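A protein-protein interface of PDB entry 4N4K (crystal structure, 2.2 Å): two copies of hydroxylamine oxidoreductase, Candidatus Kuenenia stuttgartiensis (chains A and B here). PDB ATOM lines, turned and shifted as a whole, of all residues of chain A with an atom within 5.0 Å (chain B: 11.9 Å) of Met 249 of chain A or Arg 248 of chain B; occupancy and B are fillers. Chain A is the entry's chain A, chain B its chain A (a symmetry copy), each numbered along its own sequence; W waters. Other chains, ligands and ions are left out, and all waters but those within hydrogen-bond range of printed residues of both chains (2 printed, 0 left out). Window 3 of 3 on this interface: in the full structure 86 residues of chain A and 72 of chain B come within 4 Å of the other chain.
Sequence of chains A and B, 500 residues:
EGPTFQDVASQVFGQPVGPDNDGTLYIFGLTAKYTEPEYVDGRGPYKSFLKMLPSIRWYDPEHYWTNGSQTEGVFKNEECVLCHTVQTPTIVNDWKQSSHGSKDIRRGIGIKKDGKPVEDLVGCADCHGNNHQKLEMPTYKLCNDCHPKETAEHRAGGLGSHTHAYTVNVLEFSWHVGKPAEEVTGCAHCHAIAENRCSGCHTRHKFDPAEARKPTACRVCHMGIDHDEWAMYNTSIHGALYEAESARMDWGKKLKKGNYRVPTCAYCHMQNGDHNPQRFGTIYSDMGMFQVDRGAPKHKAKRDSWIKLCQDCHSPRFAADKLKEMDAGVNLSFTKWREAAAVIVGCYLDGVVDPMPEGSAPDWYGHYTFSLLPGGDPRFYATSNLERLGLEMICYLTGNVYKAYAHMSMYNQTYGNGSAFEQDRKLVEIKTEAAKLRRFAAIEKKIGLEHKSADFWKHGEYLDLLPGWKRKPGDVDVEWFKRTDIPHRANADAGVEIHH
Of the printed residues of chain B, Lys 214 of chain A touches Ala 244 and Arg 248. Ser 246 of chain A touches just one residue of chain B: Arg 248 (2.9 Å). Printed residues of chain B within 4 Å of Arg 248 of chain A: Arg 248. Of chain B, only Arg 248 (2.9 Å) comes within 4 Å of Met 249 of chain A. No residue of chain B comes within 4 Å of Asp 250 of chain A. Of chain B, only Arg 248 (3.6 Å) comes within 4 Å of Trp 251 of chain A. No residue of chain B comes within 4 Å of Val 262 of chain A. Printed residues of chain A within 4 Å of Ala 244 of chain B: Lys 214. Printed residues of chain A within 4 Å of Ala 247 of chain B: Ala 247 (3.7 Å). Of chain A, only Lys 214, Ser 246, Ala 247, Arg 248, Met 249 and Trp 251 come within 4 Å of Arg 248 of chain B. The nearest printed residue of chain B that does not touch Lys 214 of chain A is Glu 245 of chain B (5.0 Å).
The backbone carbonyl oxygen (O) of Ser 246 of chain A sits at hydrogen-bond distance from the guanidinium group (NH2) of Arg 248 of chain B. The backbone carbonyl oxygen of Ala 247 of chain A lies within hydrogen-bond range of the guanidinium group of Arg 248 of chain B, 2.9 Å away. The guanidinium group (NH2) of Arg 248 of chain B sits at hydrogen-bond distance from the backbone carbonyl oxygen (O) of Met 249 of chain A. The backbone carbonyl oxygen of Ala 244 of chain B sits at hydrogen-bond distance from the side-chain amino group of Lys 214 of chain A (2.8 Å).
The indole nitrogen (NE1) of Trp 251 of chain A is in hydrogen-bond range of the backbone carbonyl oxygen (O) of Ser 246 of chain A (3.0 Å). OH of Tyr 260 of chain A lies within hydrogen-bond range of O of Trp 251 of chain A, 3.3 Å away.
NH1 of Arg 248 of chain B touches NZ of Lys 214 of chain A (3.9 Å). Ala 247 of chain A touches Ala 247 of chain B. Arg 248 of chain A touches Arg 248 of chain B (N to NH2, 3.7 Å). Arg 248 of chain B touches Trp 251 of chain A.
Hydrophobic or aromatic side chains of chain A within 4 Å of the printed part of chain B: Ala 247 and Trp 251. Printed residues of chain B that touch a printed residue of chain A: Ala 244, Ala 247 and Arg 248. Among the printed residues, 8 pairs touch across the chains. Among the printed residues, no Asp or Glu carboxylate lies within 4 Å of a Lys or Arg side-chain nitrogen of the other chain.
Water W1 bridges the side-chain hydroxyl (OG) of Ser 246 of chain A (2.5 Å) and the backbone carbonyl oxygen (O) of Glu 243 of chain B (3.2 Å). Water W2 lies within hydrogen-bond range of NH1 of Arg 248 of chain B, OG of Ser 246 of chain A, NZ of Lys 214 of chain A and O of Ala 244 of chain B.
Lys 214 of chain A touches Arg 248 of chain B, but with the chains exchanged Arg 248 of chain A does not touch Lys 214 of chain B (10.7 Å). Ala 247 of chain A touches Arg 248 of chain B, but with the chains exchanged Arg 248 of chain A does not touch Ala 247 of chain B (5.8 Å). Arg 248 of chain B touches its own counterpart, Arg 248 of chain A. Met 249 of chain A touches Arg 248 of chain B, but with the chains exchanged Arg 248 of chain A does not touch Met 249 of chain B (10.9 Å). Positions printed for both chains: 214, 245, 246, 247, 248, 249, 250, 251, 260 and 262. Of the 8 pairs that touch across the chains among the printed residues, 2 have their exchanged pair printed and touching as well.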
ATOM      1  N   LYS A 214     -12.661  15.464  -1.717  1.00  0.00           N
ATOM      2  CA  LYS A 214     -12.580  16.304  -0.521  1.00  0.00           C
ATOM      3  C   LYS A 214     -13.958  16.458   0.131  1.00  0.00           C
ATOM      4  O   LYS A 214     -14.960  16.475  -0.571  1.00  0.00           O
ATOM      5  CB  LYS A 214     -12.008  17.681  -0.875  1.00  0.00           C
ATOM      6  CG  LYS A 214     -10.637  17.622  -1.522  1.00  0.00           C
ATOM      7  CD  LYS A 214     -10.060  19.003  -1.830  1.00  0.00           C
ATOM      8  CE  LYS A 214      -8.859  18.876  -2.784  1.00  0.00           C
ATOM      9  NZ  LYS A 214      -7.988  20.089  -2.847  1.00  0.00           N
ATOM     10  N   GLU A 245      -4.112  18.188   7.326  1.00  0.00           N
ATOM     11  CA  GLU A 245      -3.338  17.573   6.236  1.00  0.00           C
ATOM     12  C   GLU A 245      -3.790  17.939   4.816  1.00  0.00           C
ATOM     13  O   GLU A 245      -3.057  17.689   3.866  1.00  0.00           O
ATOM     14  CB  GLU A 245      -3.334  16.046   6.393  1.00  0.00           C
ATOM     15  CG  GLU A 245      -2.713  15.564   7.701  1.00  0.00           C
ATOM     16  CD  GLU A 245      -2.350  14.080   7.708  1.00  0.00           C
ATOM     17  OE1 GLU A 245      -1.708  13.647   8.688  1.00  0.00           O
ATOM     18  OE2 GLU A 245      -2.580  13.378   6.698  1.00  0.00           O
ATOM     19  N   SER A 246      -4.918  18.631   4.677  1.00  0.00           N
ATOM     20  CA  SER A 246      -5.483  18.922   3.349  1.00  0.00           C
ATOM     21  C   SER A 246      -4.488  19.587   2.395  1.00  0.00           C
ATOM     22  O   SER A 246      -4.424  19.242   1.211  1.00  0.00           O
ATOM     23  CB  SER A 246      -6.719  19.825   3.463  1.00  0.00           C
ATOM     24  OG  SER A 246      -7.324  19.990   2.189  1.00  0.00           O
ATOM     25  N   ALA A 247      -3.766  20.577   2.911  1.00  0.00           N
ATOM     26  CA  ALA A 247      -2.888  21.415   2.099  1.00  0.00           C
ATOM     27  C   ALA A 247      -1.726  20.659   1.468  1.00  0.00           C
ATOM     28  O   ALA A 247      -1.242  21.056   0.413  1.00  0.00           O
ATOM     29  CB  ALA A 247      -2.351  22.576   2.933  1.00  0.00           C
ATOM     30  N   ARG A 248      -1.248  19.606   2.129  1.00  0.00           N
ATOM     31  CA  ARG A 248      -0.014  18.940   1.698  1.00  0.00           C
ATOM     32  C   ARG A 248      -0.172  17.470   1.298  1.00  0.00           C
ATOM     33  O   ARG A 248       0.719  16.917   0.648  1.00  0.00           O
ATOM     34  CB  ARG A 248       1.050  19.089   2.787  1.00  0.00           C
ATOM     35  CG  ARG A 248       1.428  20.553   3.046  1.00  0.00           C
ATOM     36  CD  ARG A 248       2.283  20.723   4.299  1.00  0.00           C
ATOM     37  NE  ARG A 248       2.563  22.135   4.571  1.00  0.00           N
ATOM     38  CZ  ARG A 248       1.753  22.968   5.229  1.00  0.00           C
ATOM     39  NH1 ARG A 248       0.531  22.590   5.606  1.00  0.00           N
ATOM     40  NH2 ARG A 248       2.129  24.226   5.422  1.00  0.00           N
ATOM     41  N   MET A 249      -1.356  16.905   1.524  1.00  0.00           N
ATOM     42  CA  MET A 249      -1.627  15.514   1.150  1.00  0.00           C
ATOM     43  C   MET A 249      -1.910  15.384  -0.351  1.00  0.00           C
ATOM     44  O   MET A 249      -2.334  16.342  -1.007  1.00  0.00           O
ATOM     45  CB  MET A 249      -2.797  14.939   1.971  1.00  0.00           C
ATOM     46  CG  MET A 249      -4.155  15.563   1.695  1.00  0.00           C
ATOM     47  SD  MET A 249      -5.375  15.074   2.933  1.00  0.00           S
ATOM     48  CE  MET A 249      -6.114  13.634   2.151  1.00  0.00           C
ATOM     49  N   ASP A 250      -1.766  14.164  -0.859  1.00  0.00           N
ATOM     50  CA  ASP A 250      -1.939  13.887  -2.280  1.00  0.00           C
ATOM     51  C   ASP A 250      -3.390  13.504  -2.559  1.00  0.00           C
ATOM     52  O   ASP A 250      -3.785  12.351  -2.374  1.00  0.00           O
ATOM     53  CB  ASP A 250      -0.983  12.765  -2.715  1.00  0.00           C
ATOM     54  CG  ASP A 250      -0.984  12.532  -4.232  1.00  0.00           C
ATOM     55  OD1 ASP A 250      -0.192  11.684  -4.695  1.00  0.00           O
ATOM     56  OD2 ASP A 250      -1.735  13.209  -4.967  1.00  0.00           O
ATOM     57  N   TRP A 251      -4.171  14.474  -3.030  1.00  0.00           N
ATOM     58  CA  TRP A 251      -5.570  14.243  -3.388  1.00  0.00           C
ATOM     59  C   TRP A 251      -5.716  13.578  -4.759  1.00  0.00           C
ATOM     60  O   TRP A 251      -6.830  13.283  -5.193  1.00  0.00           O
ATOM     61  CB  TRP A 251      -6.349  15.562  -3.368  1.00  0.00           C
ATOM     62  CG  TRP A 251      -6.522  16.136  -2.003  1.00  0.00           C
ATOM     63  CD1 TRP A 251      -5.884  17.225  -1.482  1.00  0.00           C
ATOM     64  CD2 TRP A 251      -7.474  15.720  -1.018  1.00  0.00           C
ATOM     65  NE1 TRP A 251      -6.405  17.533  -0.244  1.00  0.00           N
ATOM     66  CE2 TRP A 251      -7.355  16.600   0.079  1.00  0.00           C
ATOM     67  CE3 TRP A 251      -8.447  14.710  -0.972  1.00  0.00           C
ATOM     68  CZ2 TRP A 251      -8.107  16.450   1.242  1.00  0.00           C
ATOM     69  CZ3 TRP A 251      -9.199  14.564   0.187  1.00  0.00           C
ATOM     70  CH2 TRP A 251      -9.059  15.461   1.258  1.00  0.00           C
ATOM     71  N   TYR A 260      -4.820   6.665   1.556  1.00  0.00           N
ATOM     72  CA  TYR A 260      -5.110   7.826   2.404  1.00  0.00           C
ATOM     73  C   TYR A 260      -4.908   7.519   3.880  1.00  0.00           C
ATOM     74  O   TYR A 260      -5.227   6.421   4.347  1.00  0.00           O
ATOM     75  CB  TYR A 260      -6.549   8.314   2.176  1.00  0.00           C
ATOM     76  CG  TYR A 260      -6.745   9.042   0.865  1.00  0.00           C
ATOM     77  CD1 TYR A 260      -6.597  10.421   0.786  1.00  0.00           C
ATOM     78  CD2 TYR A 260      -7.066   8.350  -0.300  1.00  0.00           C
ATOM     79  CE1 TYR A 260      -6.728  11.089  -0.414  1.00  0.00           C
ATOM     80  CE2 TYR A 260      -7.192   9.011  -1.513  1.00  0.00           C
ATOM     81  CZ  TYR A 260      -6.952  10.370  -1.573  1.00  0.00           C
ATOM     82  OH  TYR A 260      -7.001  11.028  -2.777  1.00  0.00           O
ATOM     83  N   VAL A 262      -6.151   9.968   6.167  1.00  0.00           N
ATOM     84  CA  VAL A 262      -7.373  10.576   6.688  1.00  0.00           C
ATOM     85  C   VAL A 262      -8.560  10.222   5.795  1.00  0.00           C
ATOM     86  O   VAL A 262      -8.520  10.500   4.598  1.00  0.00           O
ATOM     87  CB  VAL A 262      -7.239  12.113   6.715  1.00  0.00           C
ATOM     88  CG1 VAL A 262      -8.549  12.771   7.144  1.00  0.00           C
ATOM     89  CG2 VAL A 262      -6.102  12.530   7.639  1.00  0.00           C
ATOM     90  N   ALA B 210      -1.986  39.739  -1.250  1.00  0.00           N
ATOM     91  CA  ALA B 210      -2.415  38.351  -1.466  1.00  0.00           C
ATOM     92  C   ALA B 210      -3.223  37.810  -0.278  1.00  0.00           C
ATOM     93  O   ALA B 210      -4.080  36.941  -0.447  1.00  0.00           O
ATOM     94  CB  ALA B 210      -1.207  37.452  -1.749  1.00  0.00           C
ATOM     95  N   LYS B 214      -8.073  37.025   0.249  1.00  0.00           N
ATOM     96  CA  LYS B 214      -8.711  35.831   0.804  1.00  0.00           C
ATOM     97  C   LYS B 214      -9.937  36.210   1.642  1.00  0.00           C
ATOM     98  O   LYS B 214      -9.942  37.261   2.265  1.00  0.00           O
ATOM     99  CB  LYS B 214      -7.713  35.043   1.659  1.00  0.00           C
ATOM    100  CG  LYS B 214      -6.466  34.621   0.905  1.00  0.00           C
ATOM    101  CD  LYS B 214      -5.501  33.799   1.756  1.00  0.00           C
ATOM    102  CE  LYS B 214      -4.129  33.707   1.063  1.00  0.00           C
ATOM    103  NZ  LYS B 214      -3.239  32.628   1.594  1.00  0.00           N
ATOM    104  N   ALA B 240     -17.175  26.422  -0.814  1.00  0.00           N
ATOM    105  CA  ALA B 240     -16.609  25.073  -0.769  1.00  0.00           C
ATOM    106  C   ALA B 240     -15.409  24.977  -1.699  1.00  0.00           C
ATOM    107  O   ALA B 240     -14.387  24.405  -1.337  1.00  0.00           O
ATOM    108  CB  ALA B 240     -17.654  24.027  -1.139  1.00  0.00           C
ATOM    109  N   LEU B 241     -15.511  25.580  -2.876  1.00  0.00           N
ATOM    110  CA  LEU B 241     -14.387  25.594  -3.817  1.00  0.00           C
ATOM    111  C   LEU B 241     -13.204  26.415  -3.300  1.00  0.00           C
ATOM    112  O   LEU B 241     -12.048  26.023  -3.490  1.00  0.00           O
ATOM    113  CB  LEU B 241     -14.829  26.088  -5.194  1.00  0.00           C
ATOM    114  CG  LEU B 241     -15.689  25.092  -5.976  1.00  0.00           C
ATOM    115  CD1 LEU B 241     -16.117  25.709  -7.290  1.00  0.00           C
ATOM    116  CD2 LEU B 241     -14.946  23.776  -6.220  1.00  0.00           C
ATOM    117  N   TYR B 242     -13.485  27.499  -2.578  1.00  0.00           N
ATOM    118  CA  TYR B 242     -12.422  28.260  -1.921  1.00  0.00           C
ATOM    119  C   TYR B 242     -11.661  27.370  -0.937  1.00  0.00           C
ATOM    120  O   TYR B 242     -10.429  27.370  -0.922  1.00  0.00           O
ATOM    121  CB  TYR B 242     -12.974  29.499  -1.199  1.00  0.00           C
ATOM    122  CG  TYR B 242     -12.186  29.884   0.037  1.00  0.00           C
ATOM    123  CD1 TYR B 242     -10.920  30.448  -0.071  1.00  0.00           C
ATOM    124  CD2 TYR B 242     -12.691  29.645   1.315  1.00  0.00           C
ATOM    125  CE1 TYR B 242     -10.134  30.677   1.052  1.00  0.00           C
ATOM    126  CE2 TYR B 242     -11.936  29.935   2.452  1.00  0.00           C
ATOM    127  CZ  TYR B 242     -10.640  30.412   2.306  1.00  0.00           C
ATOM    128  OH  TYR B 242      -9.862  30.658   3.411  1.00  0.00           O
ATOM    129  N   GLU B 243     -12.391  26.601  -0.132  1.00  0.00           N
ATOM    130  CA  GLU B 243     -11.749  25.714   0.840  1.00  0.00           C
ATOM    131  C   GLU B 243     -10.965  24.608   0.134  1.00  0.00           C
ATOM    132  O   GLU B 243      -9.849  24.279   0.541  1.00  0.00           O
ATOM    133  CB  GLU B 243     -12.779  25.109   1.802  1.00  0.00           C
ATOM    134  CG  GLU B 243     -12.166  24.178   2.857  1.00  0.00           C
ATOM    135  CD  GLU B 243     -13.201  23.533   3.779  1.00  0.00           C
ATOM    136  OE1 GLU B 243     -14.308  24.087   3.947  1.00  0.00           O
ATOM    137  OE2 GLU B 243     -12.865  22.501   4.400  1.00  0.00           O
ATOM    138  N   ALA B 244     -11.500  24.126  -0.985  1.00  0.00           N
ATOM    139  CA  ALA B 244     -10.847  23.069  -1.757  1.00  0.00           C
ATOM    140  C   ALA B 244      -9.567  23.544  -2.448  1.00  0.00           C
ATOM    141  O   ALA B 244      -8.576  22.824  -2.458  1.00  0.00           O
ATOM    142  CB  ALA B 244     -11.810  22.489  -2.786  1.00  0.00           C
ATOM    143  N   GLU B 245      -9.565  24.784  -2.942  1.00  0.00           N
ATOM    144  CA  GLU B 245      -8.468  25.273  -3.792  1.00  0.00           C
ATOM    145  C   GLU B 245      -7.506  26.264  -3.125  1.00  0.00           C
ATOM    146  O   GLU B 245      -6.433  26.519  -3.661  1.00  0.00           O
ATOM    147  CB  GLU B 245      -9.037  25.898  -5.074  1.00  0.00           C
ATOM    148  CG  GLU B 245      -9.852  24.925  -5.922  1.00  0.00           C
ATOM    149  CD  GLU B 245     -10.093  25.400  -7.354  1.00  0.00           C
ATOM    150  OE1 GLU B 245     -10.627  24.595  -8.147  1.00  0.00           O
ATOM    151  OE2 GLU B 245      -9.642  26.504  -7.729  1.00  0.00           O
ATOM    152  N   SER B 246      -7.820  26.724  -1.916  1.00  0.00           N
ATOM    153  CA  SER B 246      -7.015  27.765  -1.256  1.00  0.00           C
ATOM    154  C   SER B 246      -5.524  27.425  -1.178  1.00  0.00           C
ATOM    155  O   SER B 246      -4.669  28.286  -1.404  1.00  0.00           O
ATOM    156  CB  SER B 246      -7.523  28.034   0.167  1.00  0.00           C
ATOM    157  OG  SER B 246      -6.819  29.125   0.741  1.00  0.00           O
ATOM    158  N   ALA B 247      -5.234  26.184  -0.797  1.00  0.00           N
ATOM    159  CA  ALA B 247      -3.868  25.746  -0.521  1.00  0.00           C
ATOM    160  C   ALA B 247      -2.955  25.776  -1.740  1.00  0.00           C
ATOM    161  O   ALA B 247      -1.748  25.943  -1.593  1.00  0.00           O
ATOM    162  CB  ALA B 247      -3.878  24.342   0.078  1.00  0.00           C
ATOM    163  N   ARG B 248      -3.514  25.567  -2.931  1.00  0.00           N
ATOM    164  CA  ARG B 248      -2.690  25.383  -4.131  1.00  0.00           C
ATOM    165  C   ARG B 248      -2.899  26.428  -5.231  1.00  0.00           C
ATOM    166  O   ARG B 248      -2.062  26.542  -6.130  1.00  0.00           O
ATOM    167  CB  ARG B 248      -2.903  23.973  -4.683  1.00  0.00           C
ATOM    168  CG  ARG B 248      -2.464  22.881  -3.698  1.00  0.00           C
ATOM    169  CD  ARG B 248      -2.915  21.489  -4.129  1.00  0.00           C
ATOM    170  NE  ARG B 248      -2.556  20.475  -3.135  1.00  0.00           N
ATOM    171  CZ  ARG B 248      -3.272  20.174  -2.049  1.00  0.00           C
ATOM    172  NH1 ARG B 248      -4.355  20.878  -1.717  1.00  0.00           N
ATOM    173  NH2 ARG B 248      -2.843  19.222  -1.228  1.00  0.00           N
ATOM    174  N   MET B 249      -3.898  27.292  -5.064  1.00  0.00           N
ATOM    175  CA  MET B 249      -4.167  28.354  -6.037  1.00  0.00           C
ATOM    176  C   MET B 249      -3.194  29.526  -5.868  1.00  0.00           C
ATOM    177  O   MET B 249      -2.636  29.744  -4.787  1.00  0.00           O
ATOM    178  CB  MET B 249      -5.624  28.843  -5.934  1.00  0.00           C
ATOM    179  CG  MET B 249      -5.979  29.563  -4.644  1.00  0.00           C
ATOM    180  SD  MET B 249      -7.763  29.783  -4.475  1.00  0.00           S
ATOM    181  CE  MET B 249      -7.989  31.413  -5.198  1.00  0.00           C
ATOM    182  N   ASP B 250      -3.077  30.332  -6.919  1.00  0.00           N
ATOM    183  CA  ASP B 250      -2.150  31.456  -6.940  1.00  0.00           C
ATOM    184  C   ASP B 250      -2.850  32.714  -6.433  1.00  0.00           C
ATOM    185  O   ASP B 250      -3.552  33.392  -7.186  1.00  0.00           O
ATOM    186  CB  ASP B 250      -1.611  31.666  -8.364  1.00  0.00           C
ATOM    187  CG  ASP B 250      -0.499  32.722  -8.434  1.00  0.00           C
ATOM    188  OD1 ASP B 250       0.051  32.920  -9.538  1.00  0.00           O
ATOM    189  OD2 ASP B 250      -0.145  33.325  -7.399  1.00  0.00           O
ATOM    190  N   TRP B 251      -2.632  33.033  -5.158  1.00  0.00           N
ATOM    191  CA  TRP B 251      -3.197  34.236  -4.548  1.00  0.00           C
ATOM    192  C   TRP B 251      -2.407  35.496  -4.910  1.00  0.00           C
ATOM    193  O   TRP B 251      -2.775  36.599  -4.504  1.00  0.00           O
ATOM    194  CB  TRP B 251      -3.257  34.082  -3.025  1.00  0.00           C
ATOM    195  CG  TRP B 251      -4.246  33.067  -2.563  1.00  0.00           C
ATOM    196  CD1 TRP B 251      -3.977  31.829  -2.055  1.00  0.00           C
ATOM    197  CD2 TRP B 251      -5.663  33.243  -2.461  1.00  0.00           C
ATOM    198  NE1 TRP B 251      -5.139  31.235  -1.611  1.00  0.00           N
ATOM    199  CE2 TRP B 251      -6.192  32.068  -1.885  1.00  0.00           C
ATOM    200  CE3 TRP B 251      -6.536  34.299  -2.766  1.00  0.00           C
ATOM    201  CZ2 TRP B 251      -7.559  31.882  -1.687  1.00  0.00           C
ATOM    202  CZ3 TRP B 251      -7.898  34.114  -2.564  1.00  0.00           C
ATOM    203  CH2 TRP B 251      -8.390  32.933  -1.984  1.00  0.00           C
ATOM    204  N   GLY B 252      -1.282  35.323  -5.603  1.00  0.00           N
ATOM    205  CA  GLY B 252      -0.457  36.449  -6.034  1.00  0.00           C
ATOM    206  C   GLY B 252      -1.017  37.226  -7.216  1.00  0.00           C
ATOM    207  O   GLY B 252      -0.500  38.285  -7.560  1.00  0.00           O
ATOM    208  N   LYS B 253      -2.004  36.654  -7.904  1.00  0.00           N
ATOM    209  CA  LYS B 253      -2.620  37.310  -9.052  1.00  0.00           C
ATOM    210  C   LYS B 253      -3.583  38.422  -8.629  1.00  0.00           C
ATOM    211  O   LYS B 253      -4.313  38.295  -7.643  1.00  0.00           O
ATOM    212  CB  LYS B 253      -3.357  36.293  -9.928  1.00  0.00           C
ATOM    213  CG  LYS B 253      -2.448  35.313 -10.671  1.00  0.00           C
ATOM    214  CD  LYS B 253      -3.186  34.724 -11.877  1.00  0.00           C
ATOM    215  CE  LYS B 253      -2.580  33.411 -12.381  1.00  0.00           C
ATOM    216  NZ  LYS B 253      -3.589  32.606 -13.151  1.00  0.00           N
ATOM    217  N   ASN B 259      -8.254  35.866 -13.824  1.00  0.00           N
ATOM    218  CA  ASN B 259      -7.163  35.521 -12.913  1.00  0.00           C
ATOM    219  C   ASN B 259      -7.559  34.499 -11.846  1.00  0.00           C
ATOM    220  O   ASN B 259      -6.690  33.911 -11.222  1.00  0.00           O
ATOM    221  CB  ASN B 259      -6.590  36.775 -12.240  1.00  0.00           C
ATOM    222  CG  ASN B 259      -5.614  37.532 -13.127  1.00  0.00           C
ATOM    223  OD1 ASN B 259      -5.232  37.064 -14.205  1.00  0.00           O
ATOM    224  ND2 ASN B 259      -5.107  38.649 -12.613  1.00  0.00           N
ATOM    225  N   TYR B 260      -8.859  34.286 -11.646  1.00  0.00           N
ATOM    226  CA  TYR B 260      -9.338  33.387 -10.592  1.00  0.00           C
ATOM    227  C   TYR B 260     -10.464  32.488 -11.076  1.00  0.00           C
ATOM    228  O   TYR B 260     -11.328  32.917 -11.848  1.00  0.00           O
ATOM    229  CB  TYR B 260      -9.815  34.193  -9.373  1.00  0.00           C
ATOM    230  CG  TYR B 260      -8.689  34.786  -8.556  1.00  0.00           C
ATOM    231  CD1 TYR B 260      -8.140  34.088  -7.487  1.00  0.00           C
ATOM    232  CD2 TYR B 260      -8.164  36.039  -8.859  1.00  0.00           C
ATOM    233  CE1 TYR B 260      -7.082  34.601  -6.764  1.00  0.00           C
ATOM    234  CE2 TYR B 260      -7.096  36.560  -8.143  1.00  0.00           C
ATOM    235  CZ  TYR B 260      -6.516  35.803  -7.144  1.00  0.00           C
ATOM    236  OH  TYR B 260      -5.413  36.271  -6.475  1.00  0.00           O
ATOM    237  N   ARG B 261     -10.418  31.225 -10.663  1.00  0.00           N
ATOM    238  CA  ARG B 261     -11.554  30.326 -10.840  1.00  0.00           C
ATOM    239  C   ARG B 261     -12.634  30.617  -9.801  1.00  0.00           C
ATOM    240  O   ARG B 261     -13.822  30.558 -10.110  1.00  0.00           O
ATOM    241  CB  ARG B 261     -11.137  28.858 -10.728  1.00  0.00           C
ATOM    242  CG  ARG B 261     -12.336  27.911 -10.804  1.00  0.00           C
ATOM    243  CD  ARG B 261     -11.941  26.463 -10.895  1.00  0.00           C
ATOM    244  NE  ARG B 261     -13.085  25.655 -11.325  1.00  0.00           N
ATOM    245  CZ  ARG B 261     -13.587  24.603 -10.678  1.00  0.00           C
ATOM    246  NH1 ARG B 261     -12.957  24.054  -9.639  1.00  0.00           N
ATOM    247  NH2 ARG B 261     -14.650  23.989 -11.189  1.00  0.00           N
ATOM    248  N   VAL B 262     -12.213  30.674  -8.541  1.00  0.00           N
ATOM    249  CA  VAL B 262     -13.118  30.821  -7.403  1.00  0.00           C
ATOM    250  C   VAL B 262     -13.186  32.283  -6.969  1.00  0.00           C
ATOM    251  O   VAL B 262     -12.150  32.872  -6.665  1.00  0.00           O
ATOM    252  CB  VAL B 262     -12.612  29.992  -6.205  1.00  0.00           C
ATOM    253  CG1 VAL B 262     -13.479  30.227  -4.969  1.00  0.00           C
ATOM    254  CG2 VAL B 262     -12.577  28.511  -6.561  1.00  0.00           C
HETATM  255  O   HOH W   1      -9.358  21.391   1.741  1.00  0.00           O
HETATM  256  O   HOH W   2      -6.761  21.085  -0.340  1.00  0.00           O
